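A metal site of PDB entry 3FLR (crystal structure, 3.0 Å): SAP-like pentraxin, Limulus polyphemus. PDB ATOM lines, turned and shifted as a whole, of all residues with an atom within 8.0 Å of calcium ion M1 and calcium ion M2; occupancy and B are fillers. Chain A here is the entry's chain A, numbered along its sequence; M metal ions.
The nearest printed residue that does not touch calcium ion M1 is Ile 63 (4.8 Å).
Calcium ion M2 is bound by OE2 of Glu 157 (2.0 Å), OE1 of Glu 145 (2.3 Å), OD2 of Asp 147 (2.5 Å) and OD1 of Asp 147 (2.6 Å).
Slightly farther from calcium ion M2 lies OE1 of Glu 154 (3.1 Å).
Four residues have an atom within 4 Å of calcium ion M2: Glu 145, Asp 147, Glu 154 and Glu 157.
The backbone carbonyl oxygen of Ser 52 is in hydrogen-bond range of the side-chain amide nitrogen of Gln 146.
O of Glu 157 is in hydrogen-bond range of N of Tyr 49, 3.1 Å away.
N of Asp 147 lies close to O of Gly 152, at 3.4 Å.
ND2 of Asn 60 lies within hydrogen-bond range of OE1 of Gln 79 (2.6 Å).
The backbone NH of Ala 82 lies within hydrogen-bond range of the backbone carbonyl oxygen of Asn 60 (2.8 Å).
N of Asn 60 lies close to OE1 of Gln 58 (3.2 Å).
Calcium ion M1 is bound by OE2 of Glu 145 (2.2 Å), OD2 of Asp 59 (2.4 Å), OD1 of Asn 60 (2.4 Å), O of Gln 146 (2.4 Å), OD1 of Asp 147 (2.5 Å) and OE1 of Glu 145 (2.7 Å).
Calcium ion M1 has six donor atoms within binding distance.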
ATOM      1  N   TYR A  49     -15.472  25.748  20.209  1.00  0.00           N
ATOM      2  CA  TYR A  49     -14.459  24.701  20.343  1.00  0.00           C
ATOM      3  C   TYR A  49     -13.439  24.804  19.221  1.00  0.00           C
ATOM      4  O   TYR A  49     -13.808  24.976  18.062  1.00  0.00           O
ATOM      5  CB  TYR A  49     -15.109  23.315  20.339  1.00  0.00           C
ATOM      6  CG  TYR A  49     -16.086  23.096  21.469  1.00  0.00           C
ATOM      7  CD1 TYR A  49     -17.441  23.400  21.312  1.00  0.00           C
ATOM      8  CD2 TYR A  49     -15.676  22.613  22.712  1.00  0.00           C
ATOM      9  CE1 TYR A  49     -18.338  23.235  22.348  1.00  0.00           C
ATOM     10  CE2 TYR A  49     -16.570  22.436  23.754  1.00  0.00           C
ATOM     11  CZ  TYR A  49     -17.901  22.752  23.564  1.00  0.00           C
ATOM     12  OH  TYR A  49     -18.804  22.572  24.572  1.00  0.00           O
ATOM     13  N   SER A  52     -10.809  19.453  18.158  1.00  0.00           N
ATOM     14  CA  SER A  52     -11.737  18.357  18.445  1.00  0.00           C
ATOM     15  C   SER A  52     -11.179  17.005  17.999  1.00  0.00           C
ATOM     16  O   SER A  52     -10.913  16.803  16.816  1.00  0.00           O
ATOM     17  CB  SER A  52     -13.082  18.597  17.744  1.00  0.00           C
ATOM     18  OG  SER A  52     -14.013  17.551  18.019  1.00  0.00           O
ATOM     19  N   CYS A  53     -11.014  16.091  18.944  1.00  0.00           N
ATOM     20  CA  CYS A  53     -10.490  14.763  18.636  1.00  0.00           C
ATOM     21  C   CYS A  53     -11.565  13.731  18.912  1.00  0.00           C
ATOM     22  O   CYS A  53     -12.045  13.618  20.034  1.00  0.00           O
ATOM     23  CB  CYS A  53      -9.247  14.467  19.471  1.00  0.00           C
ATOM     24  SG  CYS A  53      -8.453  12.907  19.069  1.00  0.00           S
ATOM     25  N   ALA A  54     -11.921  12.972  17.886  1.00  0.00           N
ATOM     26  CA  ALA A  54     -12.975  11.976  18.016  1.00  0.00           C
ATOM     27  C   ALA A  54     -12.623  10.604  17.456  1.00  0.00           C
ATOM     28  O   ALA A  54     -11.982  10.486  16.425  1.00  0.00           O
ATOM     29  CB  ALA A  54     -14.234  12.477  17.343  1.00  0.00           C
ATOM     30  N   GLN A  58     -16.326   7.533  20.543  1.00  0.00           N
ATOM     31  CA  GLN A  58     -16.240   8.622  21.505  1.00  0.00           C
ATOM     32  C   GLN A  58     -15.893   9.883  20.740  1.00  0.00           C
ATOM     33  O   GLN A  58     -14.715  10.172  20.513  1.00  0.00           O
ATOM     34  CB  GLN A  58     -15.176   8.323  22.555  1.00  0.00           C
ATOM     35  CG  GLN A  58     -14.946   9.456  23.557  1.00  0.00           C
ATOM     36  CD  GLN A  58     -16.207   9.859  24.318  1.00  0.00           C
ATOM     37  OE1 GLN A  58     -17.173  10.365  23.743  1.00  0.00           O
ATOM     38  NE2 GLN A  58     -16.189   9.640  25.632  1.00  0.00           N
ATOM     39  N   ASP A  59     -16.914  10.625  20.337  1.00  0.00           N
ATOM     40  CA  ASP A  59     -16.747  11.858  19.594  1.00  0.00           C
ATOM     41  C   ASP A  59     -16.212  12.974  20.504  1.00  0.00           C
ATOM     42  O   ASP A  59     -15.853  14.057  20.050  1.00  0.00           O
ATOM     43  CB  ASP A  59     -18.106  12.281  19.020  1.00  0.00           C
ATOM     44  CG  ASP A  59     -19.114  12.661  20.095  1.00  0.00           C
ATOM     45  OD1 ASP A  59     -19.302  11.898  21.082  1.00  0.00           O
ATOM     46  OD2 ASP A  59     -19.731  13.749  19.957  1.00  0.00           O
ATOM     47  N   ASN A  60     -16.164  12.676  21.794  1.00  0.00           N
ATOM     48  CA  ASN A  60     -15.686  13.634  22.760  1.00  0.00           C
ATOM     49  C   ASN A  60     -14.453  13.125  23.476  1.00  0.00           C
ATOM     50  O   ASN A  60     -14.395  13.130  24.698  1.00  0.00           O
ATOM     51  CB  ASN A  60     -16.790  13.939  23.766  1.00  0.00           C
ATOM     52  CG  ASN A  60     -17.803  14.932  23.238  1.00  0.00           C
ATOM     53  OD1 ASN A  60     -18.260  14.831  22.090  1.00  0.00           O
ATOM     54  ND2 ASN A  60     -18.181  15.891  24.069  1.00  0.00           N
ATOM     55  N   GLN A  61     -13.466  12.703  22.708  1.00  0.00           N
ATOM     56  CA  GLN A  61     -12.231  12.209  23.293  1.00  0.00           C
ATOM     57  C   GLN A  61     -11.406  13.333  23.880  1.00  0.00           C
ATOM     58  O   GLN A  61     -10.899  13.216  25.005  1.00  0.00           O
ATOM     59  CB  GLN A  61     -11.437  11.458  22.239  1.00  0.00           C
ATOM     60  CG  GLN A  61     -11.886  10.021  22.063  1.00  0.00           C
ATOM     61  CD  GLN A  61     -11.235   9.101  23.071  1.00  0.00           C
ATOM     62  OE1 GLN A  61     -11.218   9.395  24.276  1.00  0.00           O
ATOM     63  NE2 GLN A  61     -10.696   7.993  22.588  1.00  0.00           N
ATOM     64  N   ILE A  63     -11.352  17.829  23.589  1.00  0.00           N
ATOM     65  CA  ILE A  63     -11.855  19.057  22.954  1.00  0.00           C
ATOM     66  C   ILE A  63     -11.430  20.326  23.664  1.00  0.00           C
ATOM     67  O   ILE A  63     -11.831  20.564  24.806  1.00  0.00           O
ATOM     68  CB  ILE A  63     -13.401  19.077  22.921  1.00  0.00           C
ATOM     69  CG1 ILE A  63     -13.957  17.655  22.845  1.00  0.00           C
ATOM     70  CG2 ILE A  63     -13.886  19.882  21.738  1.00  0.00           C
ATOM     71  CD1 ILE A  63     -15.467  17.586  22.907  1.00  0.00           C
ATOM     72  N   GLN A  79     -12.095  19.321  27.720  1.00  0.00           N
ATOM     73  CA  GLN A  79     -13.027  18.241  28.010  1.00  0.00           C
ATOM     74  C   GLN A  79     -12.354  16.949  27.578  1.00  0.00           C
ATOM     75  O   GLN A  79     -11.852  16.856  26.453  1.00  0.00           O
ATOM     76  CB  GLN A  79     -14.354  18.432  27.268  1.00  0.00           C
ATOM     77  CG  GLN A  79     -15.302  17.246  27.399  1.00  0.00           C
ATOM     78  CD  GLN A  79     -16.634  17.437  26.689  1.00  0.00           C
ATOM     79  OE1 GLN A  79     -17.412  16.490  26.520  1.00  0.00           O
ATOM     80  NE2 GLN A  79     -16.914  18.674  26.267  1.00  0.00           N
ATOM     81  N   ALA A  82     -15.704  12.632  27.110  1.00  0.00           N
ATOM     82  CA  ALA A  82     -17.076  13.064  27.342  1.00  0.00           C
ATOM     83  C   ALA A  82     -17.351  13.663  28.715  1.00  0.00           C
ATOM     84  O   ALA A  82     -18.520  13.758  29.131  1.00  0.00           O
ATOM     85  CB  ALA A  82     -18.031  11.906  27.086  1.00  0.00           C
ATOM     86  N   GLN A 144     -14.562  23.321  14.616  1.00  0.00           N
ATOM     87  CA  GLN A 144     -15.870  22.678  14.677  1.00  0.00           C
ATOM     88  C   GLN A 144     -15.793  21.570  15.698  1.00  0.00           C
ATOM     89  O   GLN A 144     -14.725  21.014  15.928  1.00  0.00           O
ATOM     90  CB  GLN A 144     -16.239  22.082  13.325  1.00  0.00           C
ATOM     91  CG  GLN A 144     -16.684  23.102  12.303  1.00  0.00           C
ATOM     92  CD  GLN A 144     -17.828  23.942  12.794  1.00  0.00           C
ATOM     93  OE1 GLN A 144     -18.541  23.570  13.735  1.00  0.00           O
ATOM     94  NE2 GLN A 144     -18.034  25.077  12.144  1.00  0.00           N
ATOM     95  N   GLU A 145     -16.927  21.234  16.297  1.00  0.00           N
ATOM     96  CA  GLU A 145     -16.986  20.199  17.318  1.00  0.00           C
ATOM     97  C   GLU A 145     -17.698  18.987  16.709  1.00  0.00           C
ATOM     98  O   GLU A 145     -18.880  19.065  16.362  1.00  0.00           O
ATOM     99  CB  GLU A 145     -17.754  20.744  18.528  1.00  0.00           C
ATOM    100  CG  GLU A 145     -17.629  19.935  19.810  1.00  0.00           C
ATOM    101  CD  GLU A 145     -18.289  18.576  19.735  1.00  0.00           C
ATOM    102  OE1 GLU A 145     -19.490  18.528  19.383  1.00  0.00           O
ATOM    103  OE2 GLU A 145     -17.617  17.563  20.022  1.00  0.00           O
ATOM    104  N   GLN A 146     -16.982  17.871  16.581  1.00  0.00           N
ATOM    105  CA  GLN A 146     -17.565  16.661  15.995  1.00  0.00           C
ATOM    106  C   GLN A 146     -18.483  15.878  16.922  1.00  0.00           C
ATOM    107  O   GLN A 146     -18.244  15.785  18.124  1.00  0.00           O
ATOM    108  CB  GLN A 146     -16.464  15.699  15.548  1.00  0.00           C
ATOM    109  CG  GLN A 146     -15.436  16.275  14.619  1.00  0.00           C
ATOM    110  CD  GLN A 146     -14.179  15.448  14.627  1.00  0.00           C
ATOM    111  OE1 GLN A 146     -14.186  14.274  14.267  1.00  0.00           O
ATOM    112  NE2 GLN A 146     -13.077  16.055  15.060  1.00  0.00           N
ATOM    113  N   ASP A 147     -19.539  15.325  16.341  1.00  0.00           N
ATOM    114  CA  ASP A 147     -20.487  14.487  17.072  1.00  0.00           C
ATOM    115  C   ASP A 147     -20.463  13.168  16.299  1.00  0.00           C
ATOM    116  O   ASP A 147     -21.031  12.158  16.699  1.00  0.00           O
ATOM    117  CB  ASP A 147     -21.901  15.069  17.044  1.00  0.00           C
ATOM    118  CG  ASP A 147     -22.089  16.216  18.009  1.00  0.00           C
ATOM    119  OD1 ASP A 147     -21.436  16.203  19.069  1.00  0.00           O
ATOM    120  OD2 ASP A 147     -22.884  17.112  17.708  1.00  0.00           O
ATOM    121  N   LYS A 148     -19.763  13.225  15.181  1.00  0.00           N
ATOM    122  CA  LYS A 148     -19.598  12.099  14.280  1.00  0.00           C
ATOM    123  C   LYS A 148     -18.142  12.257  13.790  1.00  0.00           C
ATOM    124  O   LYS A 148     -17.597  13.353  13.842  1.00  0.00           O
ATOM    125  CB  LYS A 148     -20.596  12.249  13.134  1.00  0.00           C
ATOM    126  CG  LYS A 148     -20.736  11.068  12.245  1.00  0.00           C
ATOM    127  CD  LYS A 148     -21.891  11.284  11.300  1.00  0.00           C
ATOM    128  CE  LYS A 148     -21.645  12.487  10.422  1.00  0.00           C
ATOM    129  NZ  LYS A 148     -22.753  12.693   9.425  1.00  0.00           N
ATOM    130  N   GLY A 151     -17.589  15.018  11.347  1.00  0.00           N
ATOM    131  CA  GLY A 151     -18.907  15.540  11.021  1.00  0.00           C
ATOM    132  C   GLY A 151     -19.863  15.744  12.190  1.00  0.00           C
ATOM    133  O   GLY A 151     -19.479  15.652  13.361  1.00  0.00           O
ATOM    134  N   GLY A 152     -21.123  16.017  11.891  1.00  0.00           N
ATOM    135  CA  GLY A 152     -22.098  16.253  12.939  1.00  0.00           C
ATOM    136  C   GLY A 152     -21.768  17.551  13.644  1.00  0.00           C
ATOM    137  O   GLY A 152     -21.647  17.598  14.864  1.00  0.00           O
ATOM    138  N   PHE A 153     -21.631  18.623  12.877  1.00  0.00           N
ATOM    139  CA  PHE A 153     -21.309  19.916  13.447  1.00  0.00           C
ATOM    140  C   PHE A 153     -22.540  20.692  13.887  1.00  0.00           C
ATOM    141  O   PHE A 153     -23.603  20.610  13.260  1.00  0.00           O
ATOM    142  CB  PHE A 153     -20.512  20.763  12.435  1.00  0.00           C
ATOM    143  CG  PHE A 153     -19.272  20.095  11.903  1.00  0.00           C
ATOM    144  CD1 PHE A 153     -18.436  19.361  12.740  1.00  0.00           C
ATOM    145  CD2 PHE A 153     -18.923  20.219  10.560  1.00  0.00           C
ATOM    146  CE1 PHE A 153     -17.277  18.762  12.245  1.00  0.00           C
ATOM    147  CE2 PHE A 153     -17.759  19.627  10.063  1.00  0.00           C
ATOM    148  CZ  PHE A 153     -16.949  18.903  10.912  1.00  0.00           C
ATOM    149  N   GLU A 154     -22.401  21.423  14.981  1.00  0.00           N
ATOM    150  CA  GLU A 154     -23.481  22.243  15.521  1.00  0.00           C
ATOM    151  C   GLU A 154     -22.993  23.683  15.480  1.00  0.00           C
ATOM    152  O   GLU A 154     -22.038  24.047  16.165  1.00  0.00           O
ATOM    153  CB  GLU A 154     -23.822  21.822  16.955  1.00  0.00           C
ATOM    154  CG  GLU A 154     -24.247  20.373  17.084  1.00  0.00           C
ATOM    155  CD  GLU A 154     -25.073  20.099  18.324  1.00  0.00           C
ATOM    156  OE1 GLU A 154     -24.524  20.139  19.445  1.00  0.00           O
ATOM    157  OE2 GLU A 154     -26.295  19.856  18.180  1.00  0.00           O
ATOM    158  N   GLU A 155     -23.634  24.508  14.664  1.00  0.00           N
ATOM    159  CA  GLU A 155     -23.257  25.899  14.515  1.00  0.00           C
ATOM    160  C   GLU A 155     -23.046  26.659  15.818  1.00  0.00           C
ATOM    161  O   GLU A 155     -22.250  27.600  15.872  1.00  0.00           O
ATOM    162  CB  GLU A 155     -24.319  26.619  13.682  1.00  0.00           C
ATOM    163  CG  GLU A 155     -25.718  26.267  14.116  1.00  0.00           C
ATOM    164  CD  GLU A 155     -26.745  27.256  13.633  1.00  0.00           C
ATOM    165  OE1 GLU A 155     -26.860  27.429  12.405  1.00  0.00           O
ATOM    166  OE2 GLU A 155     -27.424  27.861  14.500  1.00  0.00           O
ATOM    167  N   GLN A 156     -23.748  26.260  16.877  1.00  0.00           N
ATOM    168  CA  GLN A 156     -23.611  26.943  18.161  1.00  0.00           C
ATOM    169  C   GLN A 156     -22.317  26.569  18.888  1.00  0.00           C
ATOM    170  O   GLN A 156     -21.918  27.238  19.830  1.00  0.00           O
ATOM    171  CB  GLN A 156     -24.794  26.595  19.058  1.00  0.00           C
ATOM    172  CG  GLN A 156     -24.571  25.325  19.864  1.00  0.00           C
ATOM    173  CD  GLN A 156     -25.547  24.211  19.526  1.00  0.00           C
ATOM    174  OE1 GLN A 156     -25.813  23.917  18.358  1.00  0.00           O
ATOM    175  NE2 GLN A 156     -26.062  23.574  20.572  1.00  0.00           N
ATOM    176  N   GLU A 157     -21.674  25.487  18.454  1.00  0.00           N
ATOM    177  CA  GLU A 157     -20.438  25.045  19.094  1.00  0.00           C
ATOM    178  C   GLU A 157     -19.195  25.396  18.280  1.00  0.00           C
ATOM    179  O   GLU A 157     -18.085  25.184  18.737  1.00  0.00           O
ATOM    180  CB  GLU A 157     -20.461  23.537  19.334  1.00  0.00           C
ATOM    181  CG  GLU A 157     -21.793  23.009  19.810  1.00  0.00           C
ATOM    182  CD  GLU A 157     -21.684  21.685  20.531  1.00  0.00           C
ATOM    183  OE1 GLU A 157     -21.498  21.691  21.775  1.00  0.00           O
ATOM    184  OE2 GLU A 157     -21.773  20.639  19.865  1.00  0.00           O
ATOM    185  N   SER A 158     -19.396  25.929  17.080  1.00  0.00           N
ATOM    186  CA  SER A 158     -18.278  26.307  16.220  1.00  0.00           C
ATOM    187  C   SER A 158     -17.482  27.482  16.822  1.00  0.00           C
ATOM    188  O   SER A 158     -17.974  28.175  17.721  1.00  0.00           O
ATOM    189  CB  SER A 158     -18.802  26.709  14.837  1.00  0.00           C
ATOM    190  OG  SER A 158     -19.550  27.897  14.912  1.00  0.00           O
HETATM  191 CA    CA M   1     -19.243  16.032  20.290  1.00  0.00          CA
HETATM  192 CA    CA M   2     -21.794  18.752  19.249  1.00  0.00          CA
